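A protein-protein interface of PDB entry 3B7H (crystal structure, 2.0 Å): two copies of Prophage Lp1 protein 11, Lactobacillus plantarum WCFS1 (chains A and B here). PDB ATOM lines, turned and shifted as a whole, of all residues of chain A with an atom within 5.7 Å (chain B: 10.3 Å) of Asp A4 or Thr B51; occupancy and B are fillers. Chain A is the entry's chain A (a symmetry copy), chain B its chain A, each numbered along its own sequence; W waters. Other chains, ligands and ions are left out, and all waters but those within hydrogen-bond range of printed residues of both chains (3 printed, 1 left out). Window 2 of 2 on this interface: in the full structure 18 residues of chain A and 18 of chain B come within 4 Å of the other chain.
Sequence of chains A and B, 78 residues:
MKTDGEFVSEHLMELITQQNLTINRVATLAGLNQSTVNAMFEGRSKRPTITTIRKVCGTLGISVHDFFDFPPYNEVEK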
ATOM      1  N   LYS A   2     -12.548  28.210  16.466  1.00  0.00           N
ATOM      2  CA  LYS A   2     -11.072  28.278  16.418  1.00  0.00           C
ATOM      3  C   LYS A   2     -10.462  26.882  16.494  1.00  0.00           C
ATOM      4  O   LYS A   2     -10.854  26.073  17.313  1.00  0.00           O
ATOM      5  CB  LYS A   2     -10.503  29.078  17.592  1.00  0.00           C
ATOM      6  CG  LYS A   2     -10.564  30.562  17.490  1.00  0.00           C
ATOM      7  CD  LYS A   2      -9.914  31.151  18.746  1.00  0.00           C
ATOM      8  CE  LYS A   2     -10.039  32.675  18.784  1.00  0.00           C
ATOM      9  NZ  LYS A   2      -9.512  33.259  20.057  1.00  0.00           N
ATOM     10  N   THR A   3      -9.474  26.633  15.653  1.00  0.00           N
ATOM     11  CA  THR A   3      -8.701  25.415  15.691  1.00  0.00           C
ATOM     12  C   THR A   3      -7.742  25.444  16.872  1.00  0.00           C
ATOM     13  O   THR A   3      -7.526  26.484  17.475  1.00  0.00           O
ATOM     14  CB  THR A   3      -7.896  25.234  14.403  1.00  0.00           C
ATOM     15  OG1 THR A   3      -6.843  26.203  14.342  1.00  0.00           O
ATOM     16  CG2 THR A   3      -8.797  25.366  13.179  1.00  0.00           C
ATOM     17  N   ASP A   4      -7.177  24.293  17.206  1.00  0.00           N
ATOM     18  CA  ASP A   4      -6.177  24.225  18.259  1.00  0.00           C
ATOM     19  C   ASP A   4      -4.959  25.035  17.855  1.00  0.00           C
ATOM     20  O   ASP A   4      -4.434  25.776  18.656  1.00  0.00           O
ATOM     21  CB  ASP A   4      -5.757  22.787  18.574  1.00  0.00           C
ATOM     22  CG  ASP A   4      -6.817  22.005  19.320  1.00  0.00           C
ATOM     23  OD1 ASP A   4      -7.154  22.344  20.471  1.00  0.00           O
ATOM     24  OD2 ASP A   4      -7.287  21.014  18.758  1.00  0.00           O
ATOM     25  N   GLY A   5      -4.520  24.916  16.603  1.00  0.00           N
ATOM     26  CA  GLY A   5      -3.464  25.791  16.084  1.00  0.00           C
ATOM     27  C   GLY A   5      -3.690  27.280  16.276  1.00  0.00           C
ATOM     28  O   GLY A   5      -2.769  28.025  16.588  1.00  0.00           O
ATOM     29  N   GLU A   6      -4.918  27.720  16.077  1.00  0.00           N
ATOM     30  CA  GLU A   6      -5.308  29.102  16.335  1.00  0.00           C
ATOM     31  C   GLU A   6      -5.292  29.453  17.828  1.00  0.00           C
ATOM     32  O   GLU A   6      -4.750  30.494  18.230  1.00  0.00           O
ATOM     33  CB  GLU A   6      -6.676  29.372  15.687  1.00  0.00           C
ATOM     34  CG  GLU A   6      -6.536  29.413  14.192  1.00  0.00           C
ATOM     35  CD  GLU A   6      -7.848  29.421  13.407  1.00  0.00           C
ATOM     36  OE1 GLU A   6      -8.883  28.882  13.881  1.00  0.00           O
ATOM     37  OE2 GLU A   6      -7.811  29.973  12.284  1.00  0.00           O
ATOM     38  N   PHE A   7      -5.843  28.600  18.675  1.00  0.00           N
ATOM     39  CA  PHE A   7      -5.768  28.882  20.107  1.00  0.00           C
ATOM     40  C   PHE A   7      -4.316  28.988  20.551  1.00  0.00           C
ATOM     41  O   PHE A   7      -3.937  29.927  21.253  1.00  0.00           O
ATOM     42  CB  PHE A   7      -6.431  27.794  20.946  1.00  0.00           C
ATOM     43  CG  PHE A   7      -7.917  27.923  21.072  1.00  0.00           C
ATOM     44  CD1 PHE A   7      -8.476  29.045  21.613  1.00  0.00           C
ATOM     45  CD2 PHE A   7      -8.747  26.897  20.677  1.00  0.00           C
ATOM     46  CE1 PHE A   7      -9.844  29.159  21.761  1.00  0.00           C
ATOM     47  CE2 PHE A   7     -10.141  27.009  20.805  1.00  0.00           C
ATOM     48  CZ  PHE A   7     -10.675  28.129  21.358  1.00  0.00           C
ATOM     49  N   VAL A   8      -3.508  28.028  20.129  1.00  0.00           N
ATOM     50  CA  VAL A   8      -2.126  27.966  20.568  1.00  0.00           C
ATOM     51  C   VAL A   8      -1.295  29.128  20.029  1.00  0.00           C
ATOM     52  O   VAL A   8      -0.531  29.761  20.761  1.00  0.00           O
ATOM     53  CB  VAL A   8      -1.491  26.584  20.194  1.00  0.00           C
ATOM     54  CG1 VAL A   8       0.030  26.632  20.289  1.00  0.00           C
ATOM     55  CG2 VAL A   8      -2.080  25.491  21.112  1.00  0.00           C
ATOM     56  N   SER A   9      -1.425  29.407  18.737  1.00  0.00           N
ATOM     57  CA  SER A   9      -0.614  30.431  18.131  1.00  0.00           C
ATOM     58  C   SER A   9      -1.010  31.807  18.649  1.00  0.00           C
ATOM     59  O   SER A   9      -0.142  32.657  18.864  1.00  0.00           O
ATOM     60  CB  SER A   9      -0.661  30.322  16.598  1.00  0.00           C
ATOM     61  OG  SER A   9      -1.974  30.492  16.107  1.00  0.00           O
ATOM     62  N   LYS A  46      -2.129  21.644  10.625  1.00  0.00           N
ATOM     63  CA  LYS A  46      -2.258  20.808  11.822  1.00  0.00           C
ATOM     64  C   LYS A  46      -1.231  21.194  12.935  1.00  0.00           C
ATOM     65  O   LYS A  46      -1.364  20.798  14.143  1.00  0.00           O
ATOM     66  CB  LYS A  46      -2.137  19.321  11.435  1.00  0.00           C
ATOM     67  CG  LYS A  46      -3.290  18.761  10.570  1.00  0.00           C
ATOM     68  CD  LYS A  46      -3.152  17.241  10.201  1.00  0.00           C
ATOM     69  CE  LYS A  46      -4.302  16.599   9.294  1.00  0.00           C
ATOM     70  NZ  LYS A  46      -4.210  15.089   8.885  1.00  0.00           N
ATOM     71  N   PRO A  48       0.890  24.121  15.381  1.00  0.00           N
ATOM     72  CA  PRO A  48       2.102  23.579  16.018  1.00  0.00           C
ATOM     73  C   PRO A  48       1.982  22.177  16.710  1.00  0.00           C
ATOM     74  O   PRO A  48       0.898  21.781  17.167  1.00  0.00           O
ATOM     75  CB  PRO A  48       2.465  24.684  17.057  1.00  0.00           C
ATOM     76  CG  PRO A  48       1.669  25.896  16.620  1.00  0.00           C
ATOM     77  CD  PRO A  48       0.409  25.304  16.131  1.00  0.00           C
ATOM     78  N   TYR A  73      -7.805  25.147  27.418  1.00  0.00           N
ATOM     79  CA  TYR A  73      -6.938  24.038  27.787  1.00  0.00           C
ATOM     80  C   TYR A  73      -6.815  23.829  29.295  1.00  0.00           C
ATOM     81  O   TYR A  73      -6.447  22.741  29.726  1.00  0.00           O
ATOM     82  CB  TYR A  73      -5.564  24.220  27.161  1.00  0.00           C
ATOM     83  CG  TYR A  73      -5.614  24.206  25.662  1.00  0.00           C
ATOM     84  CD1 TYR A  73      -5.438  25.366  24.948  1.00  0.00           C
ATOM     85  CD2 TYR A  73      -5.910  23.041  24.961  1.00  0.00           C
ATOM     86  CE1 TYR A  73      -5.494  25.368  23.544  1.00  0.00           C
ATOM     87  CE2 TYR A  73      -5.978  23.036  23.557  1.00  0.00           C
ATOM     88  CZ  TYR A  73      -5.757  24.204  22.863  1.00  0.00           C
ATOM     89  OH  TYR A  73      -5.820  24.254  21.482  1.00  0.00           O
ATOM     90  N   VAL B   8       4.686  11.833  26.044  1.00  0.00           N
ATOM     91  CA  VAL B   8       3.249  12.037  26.072  1.00  0.00           C
ATOM     92  C   VAL B   8       2.477  10.720  26.104  1.00  0.00           C
ATOM     93  O   VAL B   8       1.536  10.549  26.883  1.00  0.00           O
ATOM     94  CB  VAL B   8       2.798  12.938  24.873  1.00  0.00           C
ATOM     95  CG1 VAL B   8       1.291  12.852  24.654  1.00  0.00           C
ATOM     96  CG2 VAL B   8       3.249  14.392  25.132  1.00  0.00           C
ATOM     97  N   LEU B  12       0.072   9.347  29.040  1.00  0.00           N
ATOM     98  CA  LEU B  12      -1.277   9.020  28.677  1.00  0.00           C
ATOM     99  C   LEU B  12      -1.620   7.586  29.080  1.00  0.00           C
ATOM    100  O   LEU B  12      -2.655   7.353  29.691  1.00  0.00           O
ATOM    101  CB  LEU B  12      -1.486   9.254  27.193  1.00  0.00           C
ATOM    102  CG  LEU B  12      -2.821   8.709  26.713  1.00  0.00           C
ATOM    103  CD1 LEU B  12      -3.976   9.391  27.447  1.00  0.00           C
ATOM    104  CD2 LEU B  12      -2.901   8.925  25.241  1.00  0.00           C
ATOM    105  N   ALA B  30     -13.012   8.498  22.391  1.00  0.00           N
ATOM    106  CA  ALA B  30     -12.476   9.766  21.914  1.00  0.00           C
ATOM    107  C   ALA B  30     -12.654   9.897  20.413  1.00  0.00           C
ATOM    108  O   ALA B  30     -12.387  10.946  19.834  1.00  0.00           O
ATOM    109  CB  ALA B  30     -11.001   9.895  22.268  1.00  0.00           C
ATOM    110  N   GLY B  31     -13.081   8.820  19.775  1.00  0.00           N
ATOM    111  CA  GLY B  31     -13.258   8.814  18.344  1.00  0.00           C
ATOM    112  C   GLY B  31     -11.993   8.878  17.510  1.00  0.00           C
ATOM    113  O   GLY B  31     -12.050   9.329  16.384  1.00  0.00           O
ATOM    114  N   LEU B  32     -10.845   8.430  17.999  1.00  0.00           N
ATOM    115  CA  LEU B  32      -9.737   8.316  17.051  1.00  0.00           C
ATOM    116  C   LEU B  32      -9.641   6.899  16.515  1.00  0.00           C
ATOM    117  O   LEU B  32     -10.138   5.927  17.107  1.00  0.00           O
ATOM    118  CB  LEU B  32      -8.392   8.846  17.559  1.00  0.00           C
ATOM    119  CG  LEU B  32      -7.947   8.745  19.015  1.00  0.00           C
ATOM    120  CD1 LEU B  32      -8.670   9.715  19.928  1.00  0.00           C
ATOM    121  CD2 LEU B  32      -8.130   7.309  19.451  1.00  0.00           C
ATOM    122  N   THR B  36      -4.282   6.388  14.257  1.00  0.00           N
ATOM    123  CA  THR B  36      -3.865   7.510  15.090  1.00  0.00           C
ATOM    124  C   THR B  36      -3.312   7.011  16.429  1.00  0.00           C
ATOM    125  O   THR B  36      -2.291   7.506  16.917  1.00  0.00           O
ATOM    126  CB  THR B  36      -5.024   8.496  15.381  1.00  0.00           C
ATOM    127  OG1 THR B  36      -5.604   8.986  14.155  1.00  0.00           O
ATOM    128  CG2 THR B  36      -4.499   9.672  16.214  1.00  0.00           C
ATOM    129  N   MET B  40       0.658   7.442  17.792  1.00  0.00           N
ATOM    130  CA  MET B  40       0.966   7.936  19.145  1.00  0.00           C
ATOM    131  C   MET B  40       2.124   7.184  19.794  1.00  0.00           C
ATOM    132  O   MET B  40       3.033   7.817  20.330  1.00  0.00           O
ATOM    133  CB  MET B  40      -0.294   7.829  20.015  1.00  0.00           C
ATOM    134  CG  MET B  40      -0.120   8.150  21.491  1.00  0.00           C
ATOM    135  SD  MET B  40      -1.696   8.746  22.194  1.00  0.00           S
ATOM    136  CE  MET B  40      -2.712   7.277  22.139  1.00  0.00           C
ATOM    137  N   LYS B  46       5.757  11.793  14.562  1.00  0.00           N
ATOM    138  CA  LYS B  46       5.685  13.158  15.092  1.00  0.00           C
ATOM    139  C   LYS B  46       4.423  13.386  15.986  1.00  0.00           C
ATOM    140  O   LYS B  46       4.324  14.391  16.769  1.00  0.00           O
ATOM    141  CB  LYS B  46       5.745  14.171  13.932  1.00  0.00           C
ATOM    142  CG  LYS B  46       7.088  14.232  13.169  1.00  0.00           C
ATOM    143  CD  LYS B  46       7.129  15.282  12.002  1.00  0.00           C
ATOM    144  CE  LYS B  46       8.484  15.389  11.158  1.00  0.00           C
ATOM    145  NZ  LYS B  46       8.577  16.411   9.974  1.00  0.00           N
ATOM    146  N   ARG B  47       3.475  12.442  15.887  1.00  0.00           N
ATOM    147  CA  ARG B  47       2.247  12.424  16.718  1.00  0.00           C
ATOM    148  C   ARG B  47       2.542  11.878  18.133  1.00  0.00           C
ATOM    149  O   ARG B  47       3.573  11.201  18.335  1.00  0.00           O
ATOM    150  CB  ARG B  47       1.148  11.609  16.016  1.00  0.00           C
ATOM    151  CG  ARG B  47       0.663  12.280  14.708  1.00  0.00           C
ATOM    152  CD  ARG B  47      -0.311  11.424  13.910  1.00  0.00           C
ATOM    153  NE  ARG B  47       0.330  10.522  12.944  1.00  0.00           N
ATOM    154  CZ  ARG B  47      -0.326   9.570  12.279  1.00  0.00           C
ATOM    155  NH1 ARG B  47       0.316   8.789  11.410  1.00  0.00           N
ATOM    156  NH2 ARG B  47      -1.630   9.373  12.484  1.00  0.00           N
ATOM    157  N   PRO B  48       1.650  12.169  19.128  1.00  0.00           N
ATOM    158  CA  PRO B  48       0.368  12.894  19.086  1.00  0.00           C
ATOM    159  C   PRO B  48       0.430  14.449  18.894  1.00  0.00           C
ATOM    160  O   PRO B  48       1.416  15.100  19.273  1.00  0.00           O
ATOM    161  CB  PRO B  48      -0.277  12.526  20.459  1.00  0.00           C
ATOM    162  CG  PRO B  48       0.514  11.329  20.944  1.00  0.00           C
ATOM    163  CD  PRO B  48       1.884  11.632  20.488  1.00  0.00           C
ATOM    164  N   THR B  49      -0.612  14.989  18.256  1.00  0.00           N
ATOM    165  CA  THR B  49      -0.820  16.426  18.145  1.00  0.00           C
ATOM    166  C   THR B  49      -1.550  16.919  19.408  1.00  0.00           C
ATOM    167  O   THR B  49      -2.110  16.133  20.159  1.00  0.00           O
ATOM    168  CB  THR B  49      -1.747  16.789  16.945  1.00  0.00           C
ATOM    169  OG1 THR B  49      -3.010  16.151  17.142  1.00  0.00           O
ATOM    170  CG2 THR B  49      -1.150  16.322  15.585  1.00  0.00           C
ATOM    171  N   ILE B  50      -1.622  18.236  19.559  1.00  0.00           N
ATOM    172  CA  ILE B  50      -2.411  18.877  20.626  1.00  0.00           C
ATOM    173  C   ILE B  50      -3.857  18.459  20.507  1.00  0.00           C
ATOM    174  O   ILE B  50      -4.505  18.204  21.511  1.00  0.00           O
ATOM    175  CB  ILE B  50      -2.324  20.410  20.560  1.00  0.00           C
ATOM    176  CG1 ILE B  50      -0.870  20.805  20.687  1.00  0.00           C
ATOM    177  CG2 ILE B  50      -3.120  21.086  21.727  1.00  0.00           C
ATOM    178  CD1 ILE B  50      -0.673  22.280  20.793  1.00  0.00           C
ATOM    179  N   THR B  51      -4.360  18.387  19.278  1.00  0.00           N
ATOM    180  CA  THR B  51      -5.740  17.966  19.022  1.00  0.00           C
ATOM    181  C   THR B  51      -6.027  16.578  19.593  1.00  0.00           C
ATOM    182  O   THR B  51      -6.988  16.381  20.342  1.00  0.00           O
ATOM    183  CB  THR B  51      -6.009  18.008  17.512  1.00  0.00           C
ATOM    184  OG1 THR B  51      -5.886  19.355  17.092  1.00  0.00           O
ATOM    185  CG2 THR B  51      -7.417  17.518  17.131  1.00  0.00           C
ATOM    186  N   THR B  52      -5.155  15.628  19.277  1.00  0.00           N
ATOM    187  CA  THR B  52      -5.304  14.273  19.771  1.00  0.00           C
ATOM    188  C   THR B  52      -5.248  14.241  21.304  1.00  0.00           C
ATOM    189  O   THR B  52      -6.098  13.620  21.953  1.00  0.00           O
ATOM    190  CB  THR B  52      -4.240  13.349  19.164  1.00  0.00           C
ATOM    191  OG1 THR B  52      -4.561  13.126  17.789  1.00  0.00           O
ATOM    192  CG2 THR B  52      -4.173  11.998  19.906  1.00  0.00           C
ATOM    193  N   ILE B  53      -4.274  14.938  21.877  1.00  0.00           N
ATOM    194  CA  ILE B  53      -4.163  15.025  23.351  1.00  0.00           C
ATOM    195  C   ILE B  53      -5.446  15.622  23.964  1.00  0.00           C
ATOM    196  O   ILE B  53      -6.008  15.093  24.937  1.00  0.00           O
ATOM    197  CB  ILE B  53      -2.924  15.851  23.759  1.00  0.00           C
ATOM    198  CG1 ILE B  53      -1.649  15.119  23.297  1.00  0.00           C
ATOM    199  CG2 ILE B  53      -2.927  16.114  25.273  1.00  0.00           C
ATOM    200  CD1 ILE B  53      -0.413  16.008  23.318  1.00  0.00           C
ATOM    201  N   ARG B  54      -5.936  16.697  23.361  1.00  0.00           N
ATOM    202  CA  ARG B  54      -7.163  17.340  23.844  1.00  0.00           C
ATOM    203  C   ARG B  54      -8.337  16.382  23.839  1.00  0.00           C
ATOM    204  O   ARG B  54      -9.101  16.319  24.796  1.00  0.00           O
ATOM    205  CB  ARG B  54      -7.478  18.583  23.018  1.00  0.00           C
ATOM    206  CG  ARG B  54      -8.796  19.244  23.421  1.00  0.00           C
ATOM    207  CD  ARG B  54      -9.154  20.485  22.635  1.00  0.00           C
ATOM    208  NE  ARG B  54      -9.107  20.274  21.187  1.00  0.00           N
ATOM    209  CZ  ARG B  54     -10.007  19.587  20.465  1.00  0.00           C
ATOM    210  NH1 ARG B  54     -11.047  18.965  21.036  1.00  0.00           N
ATOM    211  NH2 ARG B  54      -9.860  19.516  19.135  1.00  0.00           N
ATOM    212  N   LYS B  55      -8.486  15.636  22.750  1.00  0.00           N
ATOM    213  CA  LYS B  55      -9.598  14.698  22.609  1.00  0.00           C
ATOM    214  C   LYS B  55      -9.538  13.582  23.664  1.00  0.00           C
ATOM    215  O   LYS B  55     -10.550  13.235  24.264  1.00  0.00           O
ATOM    216  CB  LYS B  55      -9.612  14.077  21.189  1.00  0.00           C
ATOM    217  CG  LYS B  55     -10.013  15.066  20.062  1.00  0.00           C
ATOM    218  CD  LYS B  55      -9.845  14.473  18.657  1.00  0.00           C
ATOM    219  CE  LYS B  55     -10.522  15.360  17.605  1.00  0.00           C
ATOM    220  NZ  LYS B  55     -10.202  14.935  16.185  1.00  0.00           N
ATOM    221  N   VAL B  56      -8.354  13.004  23.865  1.00  0.00           N
ATOM    222  CA  VAL B  56      -8.168  11.987  24.903  1.00  0.00           C
ATOM    223  C   VAL B  56      -8.438  12.548  26.299  1.00  0.00           C
ATOM    224  O   VAL B  56      -9.060  11.897  27.132  1.00  0.00           O
ATOM    225  CB  VAL B  56      -6.762  11.406  24.866  1.00  0.00           C
ATOM    226  CG1 VAL B  56      -6.546  10.567  26.108  1.00  0.00           C
ATOM    227  CG2 VAL B  56      -6.597  10.572  23.627  1.00  0.00           C
ATOM    228  N   CYS B  57      -7.976  13.772  26.540  1.00  0.00           N
ATOM    229  CA  CYS B  57      -8.201  14.435  27.827  1.00  0.00           C
ATOM    230  C   CYS B  57      -9.684  14.562  28.098  1.00  0.00           C
ATOM    231  O   CYS B  57     -10.140  14.347  29.212  1.00  0.00           O
ATOM    232  CB  CYS B  57      -7.497  15.796  27.867  1.00  0.00           C
ATOM    233  SG  CYS B  57      -5.736  15.643  28.139  1.00  0.00           S
ATOM    234  N   GLY B  58     -10.445  14.865  27.058  1.00  0.00           N
ATOM    235  CA  GLY B  58     -11.886  14.978  27.187  1.00  0.00           C
ATOM    236  C   GLY B  58     -12.484  13.682  27.694  1.00  0.00           C
ATOM    237  O   GLY B  58     -13.321  13.675  28.607  1.00  0.00           O
ATOM    238  N   THR B  59     -12.041  12.584  27.101  1.00  0.00           N
ATOM    239  CA  THR B  59     -12.498  11.240  27.458  1.00  0.00           C
ATOM    240  C   THR B  59     -12.094  10.882  28.874  1.00  0.00           C
ATOM    241  O   THR B  59     -12.836  10.209  29.593  1.00  0.00           O
ATOM    242  CB  THR B  59     -11.895  10.187  26.512  1.00  0.00           C
ATOM    243  OG1 THR B  59     -12.352  10.434  25.181  1.00  0.00           O
ATOM    244  CG2 THR B  59     -12.293   8.792  26.926  1.00  0.00           C
ATOM    245  N   VAL B  64      -6.190  19.648  29.468  1.00  0.00           N
ATOM    246  CA  VAL B  64      -4.899  19.529  28.816  1.00  0.00           C
ATOM    247  C   VAL B  64      -3.825  20.125  29.710  1.00  0.00           C
ATOM    248  O   VAL B  64      -2.730  19.591  29.823  1.00  0.00           O
ATOM    249  CB  VAL B  64      -4.912  20.212  27.425  1.00  0.00           C
ATOM    250  CG1 VAL B  64      -3.492  20.487  26.896  1.00  0.00           C
ATOM    251  CG2 VAL B  64      -5.676  19.362  26.437  1.00  0.00           C
ATOM    252  N   PHE B  67      -3.138  17.475  32.195  1.00  0.00           N
ATOM    253  CA  PHE B  67      -2.395  16.443  31.472  1.00  0.00           C
ATOM    254  C   PHE B  67      -0.883  16.710  31.500  1.00  0.00           C
ATOM    255  O   PHE B  67      -0.093  15.804  31.710  1.00  0.00           O
ATOM    256  CB  PHE B  67      -2.875  16.327  30.016  1.00  0.00           C
ATOM    257  CG  PHE B  67      -2.102  15.313  29.222  1.00  0.00           C
ATOM    258  CD1 PHE B  67      -2.470  13.988  29.238  1.00  0.00           C
ATOM    259  CD2 PHE B  67      -0.956  15.676  28.549  1.00  0.00           C
ATOM    260  CE1 PHE B  67      -1.731  13.029  28.557  1.00  0.00           C
ATOM    261  CE2 PHE B  67      -0.196  14.733  27.872  1.00  0.00           C
ATOM    262  CZ  PHE B  67      -0.574  13.407  27.881  1.00  0.00           C
ATOM    263  N   PHE B  68      -0.486  17.957  31.329  1.00  0.00           N
ATOM    264  CA  PHE B  68       0.909  18.293  31.200  1.00  0.00           C
ATOM    265  C   PHE B  68       1.603  18.592  32.521  1.00  0.00           C
ATOM    266  O   PHE B  68       2.740  19.070  32.507  1.00  0.00           O
ATOM    267  CB  PHE B  68       1.083  19.469  30.237  1.00  0.00           C
ATOM    268  CG  PHE B  68       1.095  19.071  28.777  1.00  0.00           C
ATOM    269  CD1 PHE B  68       2.163  18.358  28.256  1.00  0.00           C
ATOM    270  CD2 PHE B  68       0.053  19.420  27.935  1.00  0.00           C
ATOM    271  CE1 PHE B  68       2.190  17.991  26.933  1.00  0.00           C
ATOM    272  CE2 PHE B  68       0.081  19.046  26.597  1.00  0.00           C
ATOM    273  CZ  PHE B  68       1.150  18.340  26.102  1.00  0.00           C
HETATM  274  O   HOH W   1      -8.612  20.905  28.294  1.00  0.00           O
HETATM  275  O   HOH W   2      -9.873  22.879  21.056  1.00  0.00           O
HETATM  276  O   HOH W   3      -3.820  19.212  14.367  1.00  0.00           O
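OG1 of Thr B51 sits at hydrogen-bond distance from OD2 of Asp A4 (2.7 Å). NE of Arg B54 is in salt-bridge range of OD1 of Asp A4 (2.9 Å). The backbone NH (N) of Val B64 lies within hydrogen-bond range of the backbone carbonyl oxygen (O) of Tyr A73 (3.1 Å).
The side-chain hydroxyl of Thr B49 lies close to the backbone NH of Thr B51 (3.4 Å). The side-chain carboxylate of Asp A4 sits at hydrogen-bond distance from the side-chain hydroxyl of Tyr A73.
Among the printed residues, pairs that only touch across the chains: Val A8 with Ile B50, Tyr A73 with Ile B50 and Pro A48 with Ile B50.
No residue of chain B comes within 4 Å of Gly A5. Val A8 touches just one residue of chain B: Ile B50. Ser A9 touches none of the printed residues of chain B. Of the printed residues of chain B, Pro A48 touches Ile B50 (3.98 Å). Of the printed residues of chain B, Tyr A73 touches Ile B50 and Val B64. Of the printed residues of chain A, Ile B50 touches Val A8 (3.5 Å), Pro A48 (3.98 Å) and Tyr A73 (3.9 Å). Of chain A, only Asp A4 (2.7 Å) comes within 4 Å of Thr B51. Ile B53 touches none of the printed residues of chain A. Of the printed residues of chain A, Arg B54 touches Asp A4. Of the printed residues of chain A, Val B64 touches Tyr A73. The nearest residue of chain B that does not touch Asp A4 is Ile B50 (4.4 Å). The nearest residue of chain A that does not touch Thr B51 is Lys A46 (5.6 Å).
Along chain A the printed residues that touch a printed residue of chain B span positions 4 to 73. Of the 24 printed residues of chain B, 4 touch a printed residue of chain A. Hydrophobic or aromatic side chains of chain B that line the printed part of chain A: Ile B50 and Val B64. Along chain B the printed residues that touch a printed residue of chain A span positions 50 to 64. Among the printed residues, 6 pairs touch across the chains.
3 positions are printed for both chains. Of the 6 pairs that touch across the chains among the printed residues, none has its exchanged pair printed and touching as well.
Water W2 bridges NE of Arg B54 (2.7 Å) and OD1 of Asp A4 (2.8 Å). Water W3 lies within hydrogen-bond range of O of Lys A46 (2.9 Å) and OG1 of Thr B51 (3.4 Å). Water W1 bridges the backbone NH (N) of Val B64 (3.0 Å) and the backbone carbonyl oxygen (O) of Tyr A73 (3.2 Å).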
